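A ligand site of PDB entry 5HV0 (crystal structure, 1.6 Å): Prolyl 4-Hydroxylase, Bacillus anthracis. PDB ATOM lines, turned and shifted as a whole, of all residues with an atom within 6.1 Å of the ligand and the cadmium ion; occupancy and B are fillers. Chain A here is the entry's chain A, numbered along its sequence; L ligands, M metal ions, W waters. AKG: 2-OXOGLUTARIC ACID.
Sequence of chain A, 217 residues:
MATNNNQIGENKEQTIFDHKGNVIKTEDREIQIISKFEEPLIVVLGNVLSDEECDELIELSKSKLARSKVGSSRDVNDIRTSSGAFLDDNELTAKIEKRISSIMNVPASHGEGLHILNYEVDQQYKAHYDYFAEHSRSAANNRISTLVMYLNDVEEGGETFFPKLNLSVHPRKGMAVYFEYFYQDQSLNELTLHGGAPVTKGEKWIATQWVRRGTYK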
ATOM      1  N   HIS A 115      15.896   5.847 -13.390  1.00  0.00           N
ATOM      2  CA  HIS A 115      14.597   5.653 -12.764  1.00  0.00           C
ATOM      3  C   HIS A 115      13.555   6.191 -13.725  1.00  0.00           C
ATOM      4  O   HIS A 115      13.627   7.354 -14.140  1.00  0.00           O
ATOM      5  CB  HIS A 115      14.530   6.426 -11.436  1.00  0.00           C
ATOM      6  CG  HIS A 115      13.237   6.259 -10.708  1.00  0.00           C
ATOM      7  ND1 HIS A 115      12.168   7.121 -10.873  1.00  0.00           N
ATOM      8  CD2 HIS A 115      12.837   5.342  -9.795  1.00  0.00           C
ATOM      9  CE1 HIS A 115      11.174   6.729 -10.098  1.00  0.00           C
ATOM     10  NE2 HIS A 115      11.554   5.657  -9.431  1.00  0.00           N
ATOM     11  N   LEU A 117       9.625   7.084 -14.745  1.00  0.00           N
ATOM     12  CA  LEU A 117       8.344   7.464 -14.170  1.00  0.00           C
ATOM     13  C   LEU A 117       7.376   7.850 -15.278  1.00  0.00           C
ATOM     14  O   LEU A 117       7.745   8.541 -16.235  1.00  0.00           O
ATOM     15  CB  LEU A 117       8.524   8.623 -13.189  1.00  0.00           C
ATOM     16  CG  LEU A 117       7.318   9.097 -12.391  1.00  0.00           C
ATOM     17  CD1 LEU A 117       6.778   7.982 -11.491  1.00  0.00           C
ATOM     18  CD2 LEU A 117       7.694  10.315 -11.566  1.00  0.00           C
ATOM     19  N   TYR A 119       3.576   9.599 -15.803  1.00  0.00           N
ATOM     20  CA  TYR A 119       2.433  10.307 -15.249  1.00  0.00           C
ATOM     21  C   TYR A 119       1.268  10.199 -16.223  1.00  0.00           C
ATOM     22  O   TYR A 119       1.434  10.442 -17.415  1.00  0.00           O
ATOM     23  CB  TYR A 119       2.699  11.799 -15.119  1.00  0.00           C
ATOM     24  CG  TYR A 119       3.799  12.247 -14.211  1.00  0.00           C
ATOM     25  CD1 TYR A 119       5.111  12.232 -14.644  1.00  0.00           C
ATOM     26  CD2 TYR A 119       3.511  12.808 -12.971  1.00  0.00           C
ATOM     27  CE1 TYR A 119       6.128  12.679 -13.838  1.00  0.00           C
ATOM     28  CE2 TYR A 119       4.524  13.272 -12.161  1.00  0.00           C
ATOM     29  CZ  TYR A 119       5.838  13.202 -12.597  1.00  0.00           C
ATOM     30  OH  TYR A 119       6.856  13.660 -11.805  1.00  0.00           O
ATOM     31  N   TYR A 125       3.671  15.424  -9.214  1.00  0.00           N
ATOM     32  CA  TYR A 125       4.670  15.135  -8.195  1.00  0.00           C
ATOM     33  C   TYR A 125       4.753  16.409  -7.347  1.00  0.00           C
ATOM     34  O   TYR A 125       5.303  17.424  -7.795  1.00  0.00           O
ATOM     35  CB  TYR A 125       6.010  14.807  -8.845  1.00  0.00           C
ATOM     36  CG  TYR A 125       6.933  13.967  -8.008  1.00  0.00           C
ATOM     37  CD1 TYR A 125       6.746  13.832  -6.628  1.00  0.00           C
ATOM     38  CD2 TYR A 125       8.004  13.293  -8.585  1.00  0.00           C
ATOM     39  CE1 TYR A 125       7.606  13.067  -5.869  1.00  0.00           C
ATOM     40  CE2 TYR A 125       8.864  12.528  -7.825  1.00  0.00           C
ATOM     41  CZ  TYR A 125       8.661  12.418  -6.480  1.00  0.00           C
ATOM     42  OH  TYR A 125       9.517  11.643  -5.729  1.00  0.00           O
ATOM     43  N   HIS A 128       9.140  18.903  -3.610  1.00  0.00           N
ATOM     44  CA  HIS A 128       9.952  18.166  -2.655  1.00  0.00           C
ATOM     45  C   HIS A 128      11.423  18.447  -2.917  1.00  0.00           C
ATOM     46  O   HIS A 128      11.797  19.092  -3.901  1.00  0.00           O
ATOM     47  CB  HIS A 128       9.707  16.670  -2.778  1.00  0.00           C
ATOM     48  CG  HIS A 128       9.959  16.144  -4.151  1.00  0.00           C
ATOM     49  ND1 HIS A 128       9.068  16.312  -5.185  1.00  0.00           N
ATOM     50  CD2 HIS A 128      11.026  15.490  -4.669  1.00  0.00           C
ATOM     51  CE1 HIS A 128       9.554  15.761  -6.291  1.00  0.00           C
ATOM     52  NE2 HIS A 128      10.734  15.247  -5.997  1.00  0.00           N
ATOM     53  N   TYR A 129      12.273  17.951  -2.007  1.00  0.00           N
ATOM     54  CA  TYR A 129      13.719  17.957  -2.174  1.00  0.00           C
ATOM     55  C   TYR A 129      14.193  16.567  -2.558  1.00  0.00           C
ATOM     56  O   TYR A 129      13.610  15.564  -2.135  1.00  0.00           O
ATOM     57  CB  TYR A 129      14.418  18.338  -0.864  1.00  0.00           C
ATOM     58  CG  TYR A 129      14.081  19.733  -0.417  1.00  0.00           C
ATOM     59  CD1 TYR A 129      14.512  20.819  -1.145  1.00  0.00           C
ATOM     60  CD2 TYR A 129      13.327  19.949   0.727  1.00  0.00           C
ATOM     61  CE1 TYR A 129      14.198  22.099  -0.752  1.00  0.00           C
ATOM     62  CE2 TYR A 129      12.997  21.230   1.125  1.00  0.00           C
ATOM     63  CZ  TYR A 129      13.447  22.299   0.387  1.00  0.00           C
ATOM     64  OH  TYR A 129      13.143  23.583   0.771  1.00  0.00           O
ATOM     65  N   ASP A 130      15.269  16.496  -3.320  1.00  0.00           N
ATOM     66  CA  ASP A 130      15.800  15.201  -3.718  1.00  0.00           C
ATOM     67  C   ASP A 130      16.830  14.688  -2.725  1.00  0.00           C
ATOM     68  O   ASP A 130      16.984  13.525  -2.602  1.00  0.00           O
ATOM     69  CB  ASP A 130      16.339  15.202  -5.186  1.00  0.00           C
ATOM     70  CG  ASP A 130      15.235  15.116  -6.235  1.00  0.00           C
ATOM     71  OD1 ASP A 130      14.214  14.710  -5.827  1.00  0.00           O
ATOM     72  OD2 ASP A 130      15.513  15.398  -7.394  1.00  0.00           O
ATOM     73  N   THR A 146      20.693  16.039  -9.573  1.00  0.00           N
ATOM     74  CA  THR A 146      19.615  15.335 -10.269  1.00  0.00           C
ATOM     75  C   THR A 146      19.627  15.732 -11.735  1.00  0.00           C
ATOM     76  O   THR A 146      19.838  16.900 -12.064  1.00  0.00           O
ATOM     77  CB  THR A 146      18.267  15.732  -9.677  1.00  0.00           C
ATOM     78  OG1 THR A 146      18.216  15.364  -8.299  1.00  0.00           O
ATOM     79  CG2 THR A 146      17.112  15.065 -10.431  1.00  0.00           C
ATOM     80  N   VAL A 148      16.798  15.213 -14.813  1.00  0.00           N
ATOM     81  CA  VAL A 148      15.485  14.727 -15.237  1.00  0.00           C
ATOM     82  C   VAL A 148      15.428  14.811 -16.753  1.00  0.00           C
ATOM     83  O   VAL A 148      15.592  15.899 -17.312  1.00  0.00           O
ATOM     84  CB  VAL A 148      14.353  15.537 -14.582  1.00  0.00           C
ATOM     85  CG1 VAL A 148      12.998  15.142 -15.169  1.00  0.00           C
ATOM     86  CG2 VAL A 148      14.353  15.316 -13.083  1.00  0.00           C
ATOM     87  N   TYR A 150      13.373  14.141 -20.310  1.00  0.00           N
ATOM     88  CA  TYR A 150      12.022  14.009 -20.851  1.00  0.00           C
ATOM     89  C   TYR A 150      12.063  12.981 -21.982  1.00  0.00           C
ATOM     90  O   TYR A 150      12.783  13.147 -22.965  1.00  0.00           O
ATOM     91  CB  TYR A 150      11.526  15.361 -21.361  1.00  0.00           C
ATOM     92  CG  TYR A 150      11.588  16.417 -20.272  1.00  0.00           C
ATOM     93  CD1 TYR A 150      10.782  16.333 -19.145  1.00  0.00           C
ATOM     94  CD2 TYR A 150      12.467  17.477 -20.369  1.00  0.00           C
ATOM     95  CE1 TYR A 150      10.845  17.291 -18.146  1.00  0.00           C
ATOM     96  CE2 TYR A 150      12.545  18.447 -19.380  1.00  0.00           C
ATOM     97  CZ  TYR A 150      11.735  18.339 -18.279  1.00  0.00           C
ATOM     98  OH  TYR A 150      11.829  19.308 -17.295  1.00  0.00           O
ATOM     99  N   GLY A 158       2.709  19.198 -17.018  1.00  0.00           N
ATOM    100  CA  GLY A 158       3.904  18.400 -16.835  1.00  0.00           C
ATOM    101  C   GLY A 158       5.192  19.179 -16.691  1.00  0.00           C
ATOM    102  O   GLY A 158       6.269  18.580 -16.830  1.00  0.00           O
ATOM    103  N   GLU A 159       5.126  20.489 -16.439  1.00  0.00           N
ATOM    104  CA  GLU A 159       6.343  21.265 -16.250  1.00  0.00           C
ATOM    105  C   GLU A 159       7.061  20.798 -14.996  1.00  0.00           C
ATOM    106  O   GLU A 159       6.444  20.400 -14.003  1.00  0.00           O
ATOM    107  CB  GLU A 159       5.994  22.745 -16.077  1.00  0.00           C
ATOM    108  CG  GLU A 159       5.241  23.366 -17.249  1.00  0.00           C
ATOM    109  CD  GLU A 159       3.728  23.337 -17.095  1.00  0.00           C
ATOM    110  OE1 GLU A 159       3.210  22.498 -16.333  1.00  0.00           O
ATOM    111  OE2 GLU A 159       3.041  24.145 -17.750  1.00  0.00           O
ATOM    112  N   THR A 160       8.394  20.842 -15.036  1.00  0.00           N
ATOM    113  CA  THR A 160       9.211  20.722 -13.832  1.00  0.00           C
ATOM    114  C   THR A 160       9.343  22.132 -13.266  1.00  0.00           C
ATOM    115  O   THR A 160       9.916  23.009 -13.925  1.00  0.00           O
ATOM    116  CB  THR A 160      10.606  20.183 -14.143  1.00  0.00           C
ATOM    117  OG1 THR A 160      10.520  18.959 -14.888  1.00  0.00           O
ATOM    118  CG2 THR A 160      11.377  19.924 -12.831  1.00  0.00           C
ATOM    119  N   PHE A 161       8.822  22.363 -12.066  1.00  0.00           N
ATOM    120  CA  PHE A 161       8.747  23.722 -11.559  1.00  0.00           C
ATOM    121  C   PHE A 161       9.510  23.840 -10.241  1.00  0.00           C
ATOM    122  O   PHE A 161       9.584  22.892  -9.457  1.00  0.00           O
ATOM    123  CB  PHE A 161       7.293  24.159 -11.364  1.00  0.00           C
ATOM    124  CG  PHE A 161       6.563  23.416 -10.293  1.00  0.00           C
ATOM    125  CD1 PHE A 161       6.072  22.136 -10.519  1.00  0.00           C
ATOM    126  CD2 PHE A 161       6.354  24.001  -9.058  1.00  0.00           C
ATOM    127  CE1 PHE A 161       5.398  21.457  -9.529  1.00  0.00           C
ATOM    128  CE2 PHE A 161       5.663  23.338  -8.067  1.00  0.00           C
ATOM    129  CZ  PHE A 161       5.186  22.059  -8.289  1.00  0.00           C
ATOM    130  N   PHE A 179      20.025  19.888 -12.010  1.00  0.00           N
ATOM    131  CA  PHE A 179      20.140  20.810 -10.883  1.00  0.00           C
ATOM    132  C   PHE A 179      20.943  20.155  -9.772  1.00  0.00           C
ATOM    133  O   PHE A 179      21.024  18.922  -9.671  1.00  0.00           O
ATOM    134  CB  PHE A 179      18.793  21.345 -10.391  1.00  0.00           C
ATOM    135  CG  PHE A 179      17.791  20.276 -10.022  1.00  0.00           C
ATOM    136  CD1 PHE A 179      17.004  19.674 -11.002  1.00  0.00           C
ATOM    137  CD2 PHE A 179      17.609  19.883  -8.698  1.00  0.00           C
ATOM    138  CE1 PHE A 179      16.078  18.709 -10.665  1.00  0.00           C
ATOM    139  CE2 PHE A 179      16.676  18.923  -8.366  1.00  0.00           C
ATOM    140  CZ  PHE A 179      15.909  18.331  -9.342  1.00  0.00           C
ATOM    141  N   HIS A 194      11.300  21.411  -5.760  1.00  0.00           N
ATOM    142  CA  HIS A 194      10.756  21.317  -7.105  1.00  0.00           C
ATOM    143  C   HIS A 194       9.728  20.226  -7.209  1.00  0.00           C
ATOM    144  O   HIS A 194       9.680  19.397  -6.414  1.00  0.00           O
ATOM    145  CB  HIS A 194      11.900  20.975  -8.097  1.00  0.00           C
ATOM    146  CG  HIS A 194      12.550  19.664  -7.794  1.00  0.00           C
ATOM    147  ND1 HIS A 194      13.437  19.498  -6.773  1.00  0.00           N
ATOM    148  CD2 HIS A 194      12.342  18.428  -8.298  1.00  0.00           C
ATOM    149  CE1 HIS A 194      13.793  18.251  -6.703  1.00  0.00           C
ATOM    150  NE2 HIS A 194      13.164  17.584  -7.634  1.00  0.00           N
ATOM    151  N   GLY A 195       8.905  20.296  -8.256  1.00  0.00           N
ATOM    152  CA  GLY A 195       7.946  19.245  -8.472  1.00  0.00           C
ATOM    153  C   GLY A 195       7.663  19.064  -9.949  1.00  0.00           C
ATOM    154  O   GLY A 195       8.238  19.729 -10.812  1.00  0.00           O
ATOM    155  N   GLY A 196       6.771  18.110 -10.220  1.00  0.00           N
ATOM    156  CA  GLY A 196       6.220  17.930 -11.550  1.00  0.00           C
ATOM    157  C   GLY A 196       4.771  18.378 -11.544  1.00  0.00           C
ATOM    158  O   GLY A 196       3.940  17.789 -10.840  1.00  0.00           O
ATOM    159  N   ALA A 197       4.472  19.399 -12.323  1.00  0.00           N
ATOM    160  CA  ALA A 197       3.124  19.928 -12.378  1.00  0.00           C
ATOM    161  C   ALA A 197       2.189  18.883 -12.994  1.00  0.00           C
ATOM    162  O   ALA A 197       2.627  18.013 -13.758  1.00  0.00           O
ATOM    163  CB  ALA A 197       3.106  21.206 -13.209  1.00  0.00           C
ATOM    164  N   LYS A 204       3.123  11.791 -19.506  1.00  0.00           N
ATOM    165  CA  LYS A 204       4.503  12.229 -19.342  1.00  0.00           C
ATOM    166  C   LYS A 204       5.362  11.033 -18.968  1.00  0.00           C
ATOM    167  O   LYS A 204       5.005  10.263 -18.069  1.00  0.00           O
ATOM    168  CB  LYS A 204       4.585  13.307 -18.255  1.00  0.00           C
ATOM    169  CG  LYS A 204       5.987  13.816 -17.931  1.00  0.00           C
ATOM    170  CD  LYS A 204       5.883  14.993 -16.946  1.00  0.00           C
ATOM    171  CE  LYS A 204       7.248  15.403 -16.404  1.00  0.00           C
ATOM    172  NZ  LYS A 204       7.080  16.454 -15.364  1.00  0.00           N
ATOM    173  N   ILE A 206       9.448  10.232 -17.919  1.00  0.00           N
ATOM    174  CA  ILE A 206      10.759  10.779 -17.603  1.00  0.00           C
ATOM    175  C   ILE A 206      11.710   9.666 -17.173  1.00  0.00           C
ATOM    176  O   ILE A 206      11.300   8.612 -16.680  1.00  0.00           O
ATOM    177  CB  ILE A 206      10.735  11.856 -16.505  1.00  0.00           C
ATOM    178  CG1 ILE A 206      10.147  11.267 -15.221  1.00  0.00           C
ATOM    179  CG2 ILE A 206       9.979  13.089 -16.980  1.00  0.00           C
ATOM    180  CD1 ILE A 206      10.311  12.152 -14.012  1.00  0.00           C
ATOM    181  N   THR A 208      15.056   9.702 -14.543  1.00  0.00           N
ATOM    182  CA  THR A 208      15.786  10.521 -13.598  1.00  0.00           C
ATOM    183  C   THR A 208      17.044   9.789 -13.186  1.00  0.00           C
ATOM    184  O   THR A 208      17.002   8.593 -12.895  1.00  0.00           O
ATOM    185  CB  THR A 208      14.963  10.815 -12.348  1.00  0.00           C
ATOM    186  OG1 THR A 208      13.713  11.396 -12.741  1.00  0.00           O
ATOM    187  CG2 THR A 208      15.709  11.801 -11.463  1.00  0.00           C
ATOM    188  N   TRP A 210      19.706  10.211 -10.150  1.00  0.00           N
ATOM    189  CA  TRP A 210      20.098  10.850  -8.899  1.00  0.00           C
ATOM    190  C   TRP A 210      21.521  10.420  -8.590  1.00  0.00           C
ATOM    191  O   TRP A 210      21.847   9.229  -8.658  1.00  0.00           O
ATOM    192  CB  TRP A 210      19.188  10.423  -7.758  1.00  0.00           C
ATOM    193  CG  TRP A 210      17.762  10.880  -7.901  1.00  0.00           C
ATOM    194  CD1 TRP A 210      17.310  12.165  -7.848  1.00  0.00           C
ATOM    195  CD2 TRP A 210      16.613  10.046  -8.093  1.00  0.00           C
ATOM    196  NE1 TRP A 210      15.946  12.186  -8.005  1.00  0.00           N
ATOM    197  CE2 TRP A 210      15.493  10.891  -8.170  1.00  0.00           C
ATOM    198  CE3 TRP A 210      16.428   8.669  -8.225  1.00  0.00           C
ATOM    199  CZ2 TRP A 210      14.203  10.414  -8.348  1.00  0.00           C
ATOM    200  CZ3 TRP A 210      15.134   8.182  -8.412  1.00  0.00           C
ATOM    201  CH2 TRP A 210      14.044   9.054  -8.478  1.00  0.00           C
HETATM  202  C1  AKG L   1      12.401  13.658  -9.874  1.00  0.00           C
HETATM  203  O1  AKG L   1      12.381  12.776 -10.765  1.00  0.00           O
HETATM  204  O2  AKG L   1      13.172  13.541  -9.025  1.00  0.00           O
HETATM  205  C2  AKG L   1      11.434  14.749 -10.039  1.00  0.00           C
HETATM  206  O5  AKG L   1      11.245  15.612  -9.349  1.00  0.00           O
HETATM  207  C3  AKG L   1      10.550  14.685 -11.313  1.00  0.00           C
HETATM  208  C4  AKG L   1      10.144  16.050 -11.865  1.00  0.00           C
HETATM  209  C5  AKG L   1       9.219  16.038 -13.070  1.00  0.00           C
HETATM  210  O3  AKG L   1       8.500  15.104 -13.195  1.00  0.00           O
HETATM  211  O4  AKG L   1       9.228  16.970 -13.824  1.00  0.00           O
HETATM  212 CD    CD M   1      12.718  15.233  -7.539  1.00  0.00          CD
HETATM  213  O   HOH W   1      11.016  10.619 -10.228  1.00  0.00           O
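OH of Tyr 119 is in hydrogen-bond range of O3 of the ligand (2.6 Å).
NZ of Lys 204 lies within salt-bridge range of O4 of the ligand, 2.7 Å away.
The side-chain hydroxyl of Thr 208 lies within hydrogen-bond range of an oxygen (O1) of the ligand, at 2.8 Å.
NE1 of Trp 210 sits close to O2 of the ligand (3.3 Å).
The side-chain hydroxyl (OG1) of Thr 160 lies within hydrogen-bond range of an oxygen (O4) of the ligand (2.6 Å).
NZ of Lys 204 sits at hydrogen-bond distance from O of Gly 158, at 2.7 Å.
The backbone NH of Tyr 125 lies within hydrogen-bond range of the backbone carbonyl oxygen of Gly 196.
The backbone carbonyl oxygen of Lys 204 is in hydrogen-bond range of the backbone NH of Tyr 119 (2.8 Å).
The backbone NH of Ile 206 is in hydrogen-bond range of the backbone carbonyl oxygen of Leu 117, 2.9 Å away.
The side-chain hydroxyl of Thr 160 sits at hydrogen-bond distance from the side-chain hydroxyl of Tyr 150, 2.8 Å away.
OD2 of Asp 130 lies within hydrogen-bond range of OG1 of Thr 146 (2.9 Å).
The backbone NH (N) of Thr 208 sits at hydrogen-bond distance from the backbone carbonyl oxygen (O) of His 115 (2.8 Å).
The side-chain carboxylate (OD2) of Asp 130 is in hydrogen-bond range of the indole nitrogen (NE1) of Trp 210 (3.3 Å).
Tyr 125 touches the ligand (CD2 to C3, 3.98 Å).
Val 148 touches the ligand.
Gly 196 touches the ligand.
Ile 206 touches the ligand.
Within 4 Å of the ligand: Tyr 119, Tyr 125, His 128, Asp 130, Val 148, Thr 160, His 194, Gly 196, Lys 204, Ile 206, Thr 208 and Trp 210.
The nearest printed residue that does not touch the ligand is Gly 195 (4.2 Å).
Of the 23 residues printed, 3 come within 4 Å of the cadmium ion.
The nearest printed residue that does not touch the cadmium ion is Trp 210 (4.5 Å).
An oxygen (O2) of the ligand is bound to the cadmium ion.
The cadmium ion is bound by the side-chain carboxylate (OD1) of Asp 130 (2.3 Å).
The cadmium ion is bound by an oxygen (O5) of the ligand, 2.4 Å away.
The cadmium ion is bound by NE2 of His 194 (2.4 Å).
NE2 of His 128 is bound to the cadmium ion (2.5 Å).
Slightly farther from the cadmium ion lies OD2 of Asp 130 (2.8 Å).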
